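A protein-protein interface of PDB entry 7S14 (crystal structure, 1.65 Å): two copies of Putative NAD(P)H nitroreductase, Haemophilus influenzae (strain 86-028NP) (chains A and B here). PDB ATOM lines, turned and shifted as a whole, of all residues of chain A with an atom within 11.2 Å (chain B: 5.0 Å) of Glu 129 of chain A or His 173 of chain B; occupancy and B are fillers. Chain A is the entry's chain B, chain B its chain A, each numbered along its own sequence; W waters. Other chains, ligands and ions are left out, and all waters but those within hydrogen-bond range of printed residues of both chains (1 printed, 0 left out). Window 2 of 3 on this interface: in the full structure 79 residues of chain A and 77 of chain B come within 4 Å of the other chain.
Among the printed residues, pairs that only touch across the chains: Asp 130 of chain A with Phe 172 of chain B, Asp 130 of chain A with His 173 of chain B, Met 131 of chain A with Tyr 174 of chain B and Lys 132 of chain A with His 173 of chain B.
No position is printed for both chains.
Glu 129 of chain A touches just one residue of chain B: His 173. His 173 of chain B touches just these residues of chain A: Glu 129, Asp 130 and Lys 132. No residue of chain A comes within 4 Å of Phe 72 of chain B. No residue of chain A comes within 4 Å of Gly 171 of chain B. No residue of chain A comes within 4 Å of Lys 176 of chain B. Printed residues of chain A within 4 Å of Tyr 174 of chain B: Asp 130 (3.1 Å) and Met 131 (3.8 Å). Printed residues of chain B within 4 Å of Asp 130 of chain A: Phe 172 (3.4 Å), His 173 (3.4 Å) and Tyr 174 (3.1 Å). Of the printed residues of chain B, Met 131 of chain A touches Tyr 174. Printed residues of chain B within 4 Å of Lys 132 of chain A: His 173 and Asp 175. Thr 139 of chain A touches none of the printed residues of chain B. Lys 122 of chain A touches none of the printed residues of chain B. The nearest residue of chain A that does not touch His 173 of chain B is Met 131 of chain A (5.8 Å). The nearest printed residue of chain B that does not touch Asp 130 of chain A is Asp 175 of chain B (4.5 Å).
Water W1 lies within hydrogen-bond range of the backbone carbonyl oxygen of Asp 130 of chain A (2.6 Å), the backbone NH of Asp 175 of chain B (3.2 Å) and the backbone carbonyl oxygen of Glu 129 of chain A (3.4 Å).
Of the 9 printed residues of chain B, 4 touch a printed residue of chain A. Of the 20 printed residues of chain A, 4 touch a printed residue of chain B. Along chain A the printed residues that touch a printed residue of chain B span positions 129 to 132. Among the printed residues, Asp or Glu carboxylates within 4 Å of a Lys or Arg side-chain nitrogen of the other chain: Lys 132 of chain A with Asp 175 of chain B (3.9 Å).
OE2 of Glu 129 of chain A lies within salt-bridge range of NZ of Lys 132 of chain A, 3.7 Å away. The backbone carbonyl oxygen of Phe 72 of chain B lies within hydrogen-bond range of the backbone NH of His 173 of chain B, at 2.9 Å. N of Lys 132 of chain A sits close to O of Gln 127 of chain A (3.4 Å). The backbone carbonyl oxygen (O) of Leu 126 of chain A lies within hydrogen-bond range of the backbone NH (N) of Met 131 of chain A, at 2.9 Å. N of Lys 176 of chain B sits close to ND1 of His 173 of chain B. O of Ala 125 of chain A is in hydrogen-bond range of N of Asp 130 of chain A.
The backbone NH of Tyr 174 of chain B sits at hydrogen-bond distance from the backbone carbonyl oxygen of Asp 130 of chain A (3.1 Å). The side-chain amino group (NZ) of Lys 132 of chain A lies within salt-bridge range of the side-chain carboxylate (OD2) of Asp 175 of chain B, at 3.9 Å. A ring nitrogen (NE2) of His 173 of chain B is in hydrogen-bond range of the side-chain carboxylate (OE2) of Glu 129 of chain A (2.9 Å).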
ATOM      1  N   ARG A  96      20.873   0.656 -27.791  1.00  0.00           N
ATOM      2  CA  ARG A  96      22.243   0.614 -27.226  1.00  0.00           C
ATOM      3  C   ARG A  96      22.388   1.782 -26.244  1.00  0.00           C
ATOM      4  O   ARG A  96      21.733   2.826 -26.457  1.00  0.00           O
ATOM      5  CB  ARG A  96      23.282   0.660 -28.352  1.00  0.00           C
ATOM      6  CG  ARG A  96      24.650   0.113 -27.972  1.00  0.00           C
ATOM      7  CD  ARG A  96      25.484  -0.239 -29.193  1.00  0.00           C
ATOM      8  NE  ARG A  96      26.756  -0.861 -28.840  1.00  0.00           N
ATOM      9  CZ  ARG A  96      27.892  -0.207 -28.593  1.00  0.00           C
ATOM     10  NH1 ARG A  96      27.942   1.113 -28.654  1.00  0.00           N
ATOM     11  NH2 ARG A  96      28.985  -0.883 -28.279  1.00  0.00           N
ATOM     12  N   TYR A  97      23.207   1.595 -25.205  1.00  0.00           N
ATOM     13  CA  TYR A  97      23.467   2.574 -24.115  1.00  0.00           C
ATOM     14  C   TYR A  97      23.920   3.924 -24.694  1.00  0.00           C
ATOM     15  O   TYR A  97      23.615   4.955 -24.070  1.00  0.00           O
ATOM     16  CB  TYR A  97      24.508   2.021 -23.137  1.00  0.00           C
ATOM     17  CG  TYR A  97      25.870   1.781 -23.739  1.00  0.00           C
ATOM     18  CD1 TYR A  97      26.226   0.545 -24.254  1.00  0.00           C
ATOM     19  CD2 TYR A  97      26.806   2.802 -23.804  1.00  0.00           C
ATOM     20  CE1 TYR A  97      27.475   0.329 -24.818  1.00  0.00           C
ATOM     21  CE2 TYR A  97      28.058   2.603 -24.365  1.00  0.00           C
ATOM     22  CZ  TYR A  97      28.396   1.361 -24.870  1.00  0.00           C
ATOM     23  OH  TYR A  97      29.629   1.166 -25.423  1.00  0.00           O
ATOM     24  N   LEU A 120      25.290   6.341 -18.030  1.00  0.00           N
ATOM     25  CA  LEU A 120      25.905   5.704 -19.229  1.00  0.00           C
ATOM     26  C   LEU A 120      26.714   4.479 -18.795  1.00  0.00           C
ATOM     27  O   LEU A 120      26.544   3.408 -19.419  1.00  0.00           O
ATOM     28  CB  LEU A 120      26.794   6.721 -19.951  1.00  0.00           C
ATOM     29  CG  LEU A 120      26.052   7.709 -20.846  1.00  0.00           C
ATOM     30  CD1 LEU A 120      26.947   8.884 -21.228  1.00  0.00           C
ATOM     31  CD2 LEU A 120      25.521   7.008 -22.088  1.00  0.00           C
ATOM     32  N   ALA A 121      27.547   4.637 -17.762  1.00  0.00           N
ATOM     33  CA  ALA A 121      28.374   3.565 -17.160  1.00  0.00           C
ATOM     34  C   ALA A 121      27.469   2.426 -16.669  1.00  0.00           C
ATOM     35  O   ALA A 121      27.845   1.258 -16.867  1.00  0.00           O
ATOM     36  CB  ALA A 121      29.218   4.134 -16.045  1.00  0.00           C
ATOM     37  N   LYS A 122      26.315   2.750 -16.073  1.00  0.00           N
ATOM     38  CA  LYS A 122      25.340   1.746 -15.558  1.00  0.00           C
ATOM     39  C   LYS A 122      24.688   1.010 -16.732  1.00  0.00           C
ATOM     40  O   LYS A 122      24.667  -0.235 -16.697  1.00  0.00           O
ATOM     41  CB  LYS A 122      24.272   2.386 -14.663  1.00  0.00           C
ATOM     42  CG  LYS A 122      24.659   2.569 -13.200  1.00  0.00           C
ATOM     43  CD  LYS A 122      25.625   1.518 -12.681  1.00  0.00           C
ATOM     44  CE  LYS A 122      25.554   1.298 -11.186  1.00  0.00           C
ATOM     45  NZ  LYS A 122      26.329   0.100 -10.784  1.00  0.00           N
ATOM     46  N   TYR A 123      24.175   1.746 -17.723  1.00  0.00           N
ATOM     47  CA  TYR A 123      23.543   1.175 -18.942  1.00  0.00           C
ATOM     48  C   TYR A 123      24.543   0.226 -19.616  1.00  0.00           C
ATOM     49  O   TYR A 123      24.152  -0.902 -19.966  1.00  0.00           O
ATOM     50  CB  TYR A 123      23.100   2.265 -19.922  1.00  0.00           C
ATOM     51  CG  TYR A 123      22.196   3.341 -19.367  1.00  0.00           C
ATOM     52  CD1 TYR A 123      21.376   3.122 -18.268  1.00  0.00           C
ATOM     53  CD2 TYR A 123      22.155   4.589 -19.963  1.00  0.00           C
ATOM     54  CE1 TYR A 123      20.547   4.118 -17.775  1.00  0.00           C
ATOM     55  CE2 TYR A 123      21.334   5.595 -19.484  1.00  0.00           C
ATOM     56  CZ  TYR A 123      20.527   5.360 -18.385  1.00  0.00           C
ATOM     57  OH  TYR A 123      19.722   6.364 -17.926  1.00  0.00           O
ATOM     58  N   LYS A 124      25.796   0.673 -19.762  1.00  0.00           N
ATOM     59  CA  LYS A 124      26.884  -0.072 -20.450  1.00  0.00           C
ATOM     60  C   LYS A 124      27.116  -1.418 -19.754  1.00  0.00           C
ATOM     61  O   LYS A 124      27.126  -2.442 -20.462  1.00  0.00           O
ATOM     62  CB  LYS A 124      28.179   0.746 -20.477  1.00  0.00           C
ATOM     63  CG  LYS A 124      29.336   0.069 -21.201  1.00  0.00           C
ATOM     64  CD  LYS A 124      30.367   1.027 -21.754  1.00  0.00           C
ATOM     65  CE  LYS A 124      31.362   0.357 -22.678  1.00  0.00           C
ATOM     66  NZ  LYS A 124      32.254  -0.581 -21.955  1.00  0.00           N
ATOM     67  N   ALA A 125      27.300  -1.415 -18.429  1.00  0.00           N
ATOM     68  CA  ALA A 125      27.556  -2.632 -17.619  1.00  0.00           C
ATOM     69  C   ALA A 125      26.382  -3.604 -17.780  1.00  0.00           C
ATOM     70  O   ALA A 125      26.635  -4.798 -18.033  1.00  0.00           O
ATOM     71  CB  ALA A 125      27.774  -2.275 -16.168  1.00  0.00           C
ATOM     72  N   LEU A 126      25.148  -3.101 -17.659  1.00  0.00           N
ATOM     73  CA  LEU A 126      23.915  -3.930 -17.724  1.00  0.00           C
ATOM     74  C   LEU A 126      23.848  -4.646 -19.078  1.00  0.00           C
ATOM     75  O   LEU A 126      23.577  -5.862 -19.088  1.00  0.00           O
ATOM     76  CB  LEU A 126      22.674  -3.056 -17.510  1.00  0.00           C
ATOM     77  CG  LEU A 126      21.350  -3.819 -17.457  1.00  0.00           C
ATOM     78  CD1 LEU A 126      21.221  -4.594 -16.151  1.00  0.00           C
ATOM     79  CD2 LEU A 126      20.172  -2.877 -17.643  1.00  0.00           C
ATOM     80  N   GLN A 127      24.074  -3.918 -20.177  1.00  0.00           N
ATOM     81  CA  GLN A 127      23.917  -4.454 -21.555  1.00  0.00           C
ATOM     82  C   GLN A 127      25.101  -5.366 -21.904  1.00  0.00           C
ATOM     83  O   GLN A 127      24.853  -6.428 -22.504  1.00  0.00           O
ATOM     84  CB  GLN A 127      23.777  -3.314 -22.563  1.00  0.00           C
ATOM     85  CG  GLN A 127      22.507  -2.499 -22.369  1.00  0.00           C
ATOM     86  CD  GLN A 127      22.185  -1.616 -23.548  1.00  0.00           C
ATOM     87  OE1 GLN A 127      23.062  -1.206 -24.307  1.00  0.00           O
ATOM     88  NE2 GLN A 127      20.909  -1.303 -23.703  1.00  0.00           N
ATOM     89  N   GLU A 128      26.327  -4.977 -21.536  1.00  0.00           N
ATOM     90  CA  GLU A 128      27.582  -5.649 -21.981  1.00  0.00           C
ATOM     91  C   GLU A 128      27.886  -6.880 -21.117  1.00  0.00           C
ATOM     92  O   GLU A 128      28.292  -7.907 -21.699  1.00  0.00           O
ATOM     93  CB  GLU A 128      28.775  -4.692 -21.939  1.00  0.00           C
ATOM     94  CG  GLU A 128      28.888  -3.817 -23.173  1.00  0.00           C
ATOM     95  CD  GLU A 128      30.164  -2.997 -23.262  1.00  0.00           C
ATOM     96  OE1 GLU A 128      30.913  -2.960 -22.264  1.00  0.00           O
ATOM     97  OE2 GLU A 128      30.409  -2.401 -24.335  1.00  0.00           O
ATOM     98  N   GLU A 129      27.724  -6.781 -19.793  1.00  0.00           N
ATOM     99  CA  GLU A 129      28.247  -7.783 -18.821  1.00  0.00           C
ATOM    100  C   GLU A 129      27.097  -8.531 -18.135  1.00  0.00           C
ATOM    101  O   GLU A 129      27.063  -9.769 -18.237  1.00  0.00           O
ATOM    102  CB  GLU A 129      29.144  -7.091 -17.789  1.00  0.00           C
ATOM    103  CG  GLU A 129      29.774  -8.039 -16.781  1.00  0.00           C
ATOM    104  CD  GLU A 129      30.690  -9.099 -17.369  1.00  0.00           C
ATOM    105  OE1 GLU A 129      31.222  -8.874 -18.475  1.00  0.00           O
ATOM    106  OE2 GLU A 129      30.869 -10.152 -16.721  1.00  0.00           O
ATOM    107  N   ASP A 130      26.198  -7.811 -17.457  1.00  0.00           N
ATOM    108  CA  ASP A 130      25.227  -8.406 -16.499  1.00  0.00           C
ATOM    109  C   ASP A 130      24.187  -9.242 -17.251  1.00  0.00           C
ATOM    110  O   ASP A 130      23.969 -10.402 -16.841  1.00  0.00           O
ATOM    111  CB  ASP A 130      24.577  -7.325 -15.637  1.00  0.00           C
ATOM    112  CG  ASP A 130      25.565  -6.666 -14.694  1.00  0.00           C
ATOM    113  OD1 ASP A 130      26.237  -7.405 -13.934  1.00  0.00           O
ATOM    114  OD2 ASP A 130      25.679  -5.425 -14.746  1.00  0.00           O
ATOM    115  N   MET A 131      23.580  -8.672 -18.299  1.00  0.00           N
ATOM    116  CA  MET A 131      22.482  -9.305 -19.079  1.00  0.00           C
ATOM    117  C   MET A 131      22.986  -9.765 -20.455  1.00  0.00           C
ATOM    118  O   MET A 131      22.245 -10.522 -21.115  1.00  0.00           O
ATOM    119  CB  MET A 131      21.313  -8.322 -19.214  1.00  0.00           C
ATOM    120  CG  MET A 131      20.799  -7.765 -17.892  1.00  0.00           C
ATOM    121  SD  MET A 131      19.035  -6.900 -18.063  1.00  0.00           S
ATOM    122  CE  MET A 131      17.841  -8.391 -18.508  1.00  0.00           C
ATOM    123  N   LYS A 132      24.177  -9.318 -20.880  1.00  0.00           N
ATOM    124  CA  LYS A 132      24.825  -9.710 -22.163  1.00  0.00           C
ATOM    125  C   LYS A 132      23.805  -9.585 -23.303  1.00  0.00           C
ATOM    126  O   LYS A 132      23.579 -10.576 -24.026  1.00  0.00           O
ATOM    127  CB  LYS A 132      25.419 -11.115 -22.033  1.00  0.00           C
ATOM    128  CG  LYS A 132      26.435 -11.253 -20.906  1.00  0.00           C
ATOM    129  CD  LYS A 132      27.314 -12.480 -20.999  1.00  0.00           C
ATOM    130  CE  LYS A 132      27.802 -12.954 -19.646  1.00  0.00           C
ATOM    131  NZ  LYS A 132      28.458 -11.873 -18.873  1.00  0.00           N
ATOM    132  N   LEU A 133      23.223  -8.392 -23.441  1.00  0.00           N
ATOM    133  CA  LEU A 133      22.156  -8.055 -24.422  1.00  0.00           C
ATOM    134  C   LEU A 133      22.773  -7.743 -25.789  1.00  0.00           C
ATOM    135  O   LEU A 133      22.016  -7.702 -26.778  1.00  0.00           O
ATOM    136  CB  LEU A 133      21.376  -6.842 -23.910  1.00  0.00           C
ATOM    137  CG  LEU A 133      20.697  -7.007 -22.552  1.00  0.00           C
ATOM    138  CD1 LEU A 133      19.985  -5.724 -22.152  1.00  0.00           C
ATOM    139  CD2 LEU A 133      19.728  -8.176 -22.566  1.00  0.00           C
ATOM    140  N   LEU A 134      24.087  -7.508 -25.843  1.00  0.00           N
ATOM    141  CA  LEU A 134      24.795  -7.070 -27.074  1.00  0.00           C
ATOM    142  C   LEU A 134      25.380  -8.288 -27.797  1.00  0.00           C
ATOM    143  O   LEU A 134      26.284  -8.096 -28.629  1.00  0.00           O
ATOM    144  CB  LEU A 134      25.882  -6.062 -26.689  1.00  0.00           C
ATOM    145  CG  LEU A 134      25.395  -4.842 -25.907  1.00  0.00           C
ATOM    146  CD1 LEU A 134      26.513  -3.830 -25.746  1.00  0.00           C
ATOM    147  CD2 LEU A 134      24.194  -4.195 -26.583  1.00  0.00           C
ATOM    148  N   GLU A 135      24.873  -9.489 -27.490  1.00  0.00           N
ATOM    149  CA  GLU A 135      25.201 -10.750 -28.206  1.00  0.00           C
ATOM    150  C   GLU A 135      24.882 -10.554 -29.692  1.00  0.00           C
ATOM    151  O   GLU A 135      25.733 -10.893 -30.530  1.00  0.00           O
ATOM    152  CB  GLU A 135      24.420 -11.921 -27.603  1.00  0.00           C
ATOM    153  CG  GLU A 135      24.771 -13.272 -28.208  1.00  0.00           C
ATOM    154  CD  GLU A 135      24.093 -14.469 -27.559  1.00  0.00           C
ATOM    155  OE1 GLU A 135      23.964 -14.481 -26.318  1.00  0.00           O
ATOM    156  OE2 GLU A 135      23.696 -15.392 -28.300  1.00  0.00           O
ATOM    157  N   THR A 139      18.822 -10.175 -29.268  1.00  0.00           N
ATOM    158  CA  THR A 139      18.935 -10.190 -27.782  1.00  0.00           C
ATOM    159  C   THR A 139      18.618  -8.793 -27.237  1.00  0.00           C
ATOM    160  O   THR A 139      17.899  -8.707 -26.220  1.00  0.00           O
ATOM    161  CB  THR A 139      20.316 -10.669 -27.321  1.00  0.00           C
ATOM    162  OG1 THR A 139      21.312  -9.841 -27.921  1.00  0.00           O
ATOM    163  CG2 THR A 139      20.571 -12.114 -27.675  1.00  0.00           C
ATOM    164  N   LEU A 140      19.117  -7.748 -27.904  1.00  0.00           N
ATOM    165  CA  LEU A 140      18.903  -6.328 -27.517  1.00  0.00           C
ATOM    166  C   LEU A 140      17.430  -5.960 -27.732  1.00  0.00           C
ATOM    167  O   LEU A 140      16.849  -5.316 -26.833  1.00  0.00           O
ATOM    168  CB  LEU A 140      19.844  -5.438 -28.338  1.00  0.00           C
ATOM    169  CG  LEU A 140      19.960  -3.975 -27.902  1.00  0.00           C
ATOM    170  CD1 LEU A 140      20.095  -3.833 -26.391  1.00  0.00           C
ATOM    171  CD2 LEU A 140      21.121  -3.291 -28.606  1.00  0.00           C
ATOM    172  N   PHE B  72      27.024  -9.023  -6.396  1.00  0.00           N
ATOM    173  CA  PHE B  72      26.736  -8.973  -7.856  1.00  0.00           C
ATOM    174  C   PHE B  72      25.316  -8.463  -8.132  1.00  0.00           C
ATOM    175  O   PHE B  72      24.890  -8.580  -9.293  1.00  0.00           O
ATOM    176  CB  PHE B  72      26.968 -10.342  -8.507  1.00  0.00           C
ATOM    177  CG  PHE B  72      26.223 -11.502  -7.893  1.00  0.00           C
ATOM    178  CD1 PHE B  72      24.871 -11.695  -8.135  1.00  0.00           C
ATOM    179  CD2 PHE B  72      26.888 -12.426  -7.099  1.00  0.00           C
ATOM    180  CE1 PHE B  72      24.196 -12.772  -7.578  1.00  0.00           C
ATOM    181  CE2 PHE B  72      26.211 -13.500  -6.542  1.00  0.00           C
ATOM    182  CZ  PHE B  72      24.868 -13.674  -6.786  1.00  0.00           C
ATOM    183  N   GLY B 171      19.034  -5.360 -12.116  1.00  0.00           N
ATOM    184  CA  GLY B 171      20.395  -4.885 -11.808  1.00  0.00           C
ATOM    185  C   GLY B 171      21.195  -5.909 -11.024  1.00  0.00           C
ATOM    186  O   GLY B 171      21.572  -5.620  -9.868  1.00  0.00           O
ATOM    187  N   PHE B 172      21.455  -7.071 -11.624  1.00  0.00           N
ATOM    188  CA  PHE B 172      22.362  -8.109 -11.072  1.00  0.00           C
ATOM    189  C   PHE B 172      23.044  -8.851 -12.222  1.00  0.00           C
ATOM    190  O   PHE B 172      22.553  -8.782 -13.368  1.00  0.00           O
ATOM    191  CB  PHE B 172      21.611  -9.079 -10.155  1.00  0.00           C
ATOM    192  CG  PHE B 172      20.404  -9.735 -10.776  1.00  0.00           C
ATOM    193  CD1 PHE B 172      20.527 -10.896 -11.526  1.00  0.00           C
ATOM    194  CD2 PHE B 172      19.140  -9.187 -10.613  1.00  0.00           C
ATOM    195  CE1 PHE B 172      19.411 -11.494 -12.094  1.00  0.00           C
ATOM    196  CE2 PHE B 172      18.028  -9.782 -11.187  1.00  0.00           C
ATOM    197  CZ  PHE B 172      18.164 -10.935 -11.926  1.00  0.00           C
ATOM    198  N   HIS B 173      24.148  -9.538 -11.917  1.00  0.00           N
ATOM    199  CA  HIS B 173      24.873 -10.405 -12.879  1.00  0.00           C
ATOM    200  C   HIS B 173      24.090 -11.713 -13.019  1.00  0.00           C
ATOM    201  O   HIS B 173      24.042 -12.491 -12.041  1.00  0.00           O
ATOM    202  CB  HIS B 173      26.328 -10.618 -12.454  1.00  0.00           C
ATOM    203  CG  HIS B 173      27.209 -11.016 -13.589  1.00  0.00           C
ATOM    204  ND1 HIS B 173      27.326 -12.325 -14.012  1.00  0.00           N
ATOM    205  CD2 HIS B 173      27.991 -10.280 -14.409  1.00  0.00           C
ATOM    206  CE1 HIS B 173      28.158 -12.379 -15.033  1.00  0.00           C
ATOM    207  NE2 HIS B 173      28.574 -11.139 -15.300  1.00  0.00           N
ATOM    208  N   TYR B 174      23.483 -11.934 -14.186  1.00  0.00           N
ATOM    209  CA  TYR B 174      22.560 -13.070 -14.438  1.00  0.00           C
ATOM    210  C   TYR B 174      23.322 -14.397 -14.362  1.00  0.00           C
ATOM    211  O   TYR B 174      22.794 -15.329 -13.736  1.00  0.00           O
ATOM    212  CB  TYR B 174      21.823 -12.892 -15.765  1.00  0.00           C
ATOM    213  CG  TYR B 174      20.539 -12.116 -15.624  1.00  0.00           C
ATOM    214  CD1 TYR B 174      20.552 -10.758 -15.347  1.00  0.00           C
ATOM    215  CD2 TYR B 174      19.310 -12.747 -15.720  1.00  0.00           C
ATOM    216  CE1 TYR B 174      19.375 -10.038 -15.205  1.00  0.00           C
ATOM    217  CE2 TYR B 174      18.125 -12.042 -15.583  1.00  0.00           C
ATOM    218  CZ  TYR B 174      18.156 -10.683 -15.317  1.00  0.00           C
ATOM    219  OH  TYR B 174      17.000  -9.969 -15.172  1.00  0.00           O
ATOM    220  N   ASP B 175      24.508 -14.474 -14.969  1.00  0.00           N
ATOM    221  CA  ASP B 175      25.359 -15.695 -14.949  1.00  0.00           C
ATOM    222  C   ASP B 175      25.658 -16.074 -13.494  1.00  0.00           C
ATOM    223  O   ASP B 175      25.496 -17.264 -13.150  1.00  0.00           O
ATOM    224  CB  ASP B 175      26.658 -15.501 -15.735  1.00  0.00           C
ATOM    225  CG  ASP B 175      26.531 -15.666 -17.240  1.00  0.00           C
ATOM    226  OD1 ASP B 175      25.413 -15.942 -17.716  1.00  0.00           O
ATOM    227  OD2 ASP B 175      27.564 -15.525 -17.927  1.00  0.00           O
ATOM    228  N   LYS B 176      26.072 -15.104 -12.673  1.00  0.00           N
ATOM    229  CA  LYS B 176      26.476 -15.338 -11.258  1.00  0.00           C
ATOM    230  C   LYS B 176      25.225 -15.595 -10.410  1.00  0.00           C
ATOM    231  O   LYS B 176      25.308 -16.404  -9.473  1.00  0.00           O
ATOM    232  CB  LYS B 176      27.291 -14.158 -10.724  1.00  0.00           C
ATOM    233  CG  LYS B 176      28.662 -13.998 -11.368  1.00  0.00           C
ATOM    234  CD  LYS B 176      29.214 -12.594 -11.328  1.00  0.00           C
ATOM    235  CE  LYS B 176      30.007 -12.278 -10.079  1.00  0.00           C
ATOM    236  NZ  LYS B 176      30.689 -10.967 -10.204  1.00  0.00           N
ATOM    237  N   MET B 177      24.108 -14.928 -10.715  1.00  0.00           N
ATOM    238  CA  MET B 177      22.818 -15.179 -10.021  1.00  0.00           C
ATOM    239  C   MET B 177      22.360 -16.613 -10.325  1.00  0.00           C
ATOM    240  O   MET B 177      21.917 -17.300  -9.378  1.00  0.00           O
ATOM    241  CB  MET B 177      21.758 -14.157 -10.442  1.00  0.00           C
ATOM    242  CG  MET B 177      20.411 -14.362  -9.778  1.00  0.00           C
ATOM    243  SD  MET B 177      20.485 -13.973  -7.854  1.00  0.00           S
ATOM    244  CE  MET B 177      20.274 -12.021  -7.731  1.00  0.00           C
ATOM    245  N   ASN B 178      22.461 -17.047 -11.587  1.00  0.00           N
ATOM    246  CA  ASN B 178      22.071 -18.413 -12.033  1.00  0.00           C
ATOM    247  C   ASN B 178      22.933 -19.450 -11.304  1.00  0.00           C
ATOM    248  O   ASN B 178      22.355 -20.405 -10.757  1.00  0.00           O
ATOM    249  CB  ASN B 178      22.180 -18.592 -13.549  1.00  0.00           C
ATOM    250  CG  ASN B 178      20.959 -18.095 -14.292  1.00  0.00           C
ATOM    251  OD1 ASN B 178      19.853 -18.590 -14.078  1.00  0.00           O
ATOM    252  ND2 ASN B 178      21.146 -17.122 -15.168  1.00  0.00           N
HETATM  253  O   HOH W   1      25.317 -12.524 -17.433  1.00  0.00           O
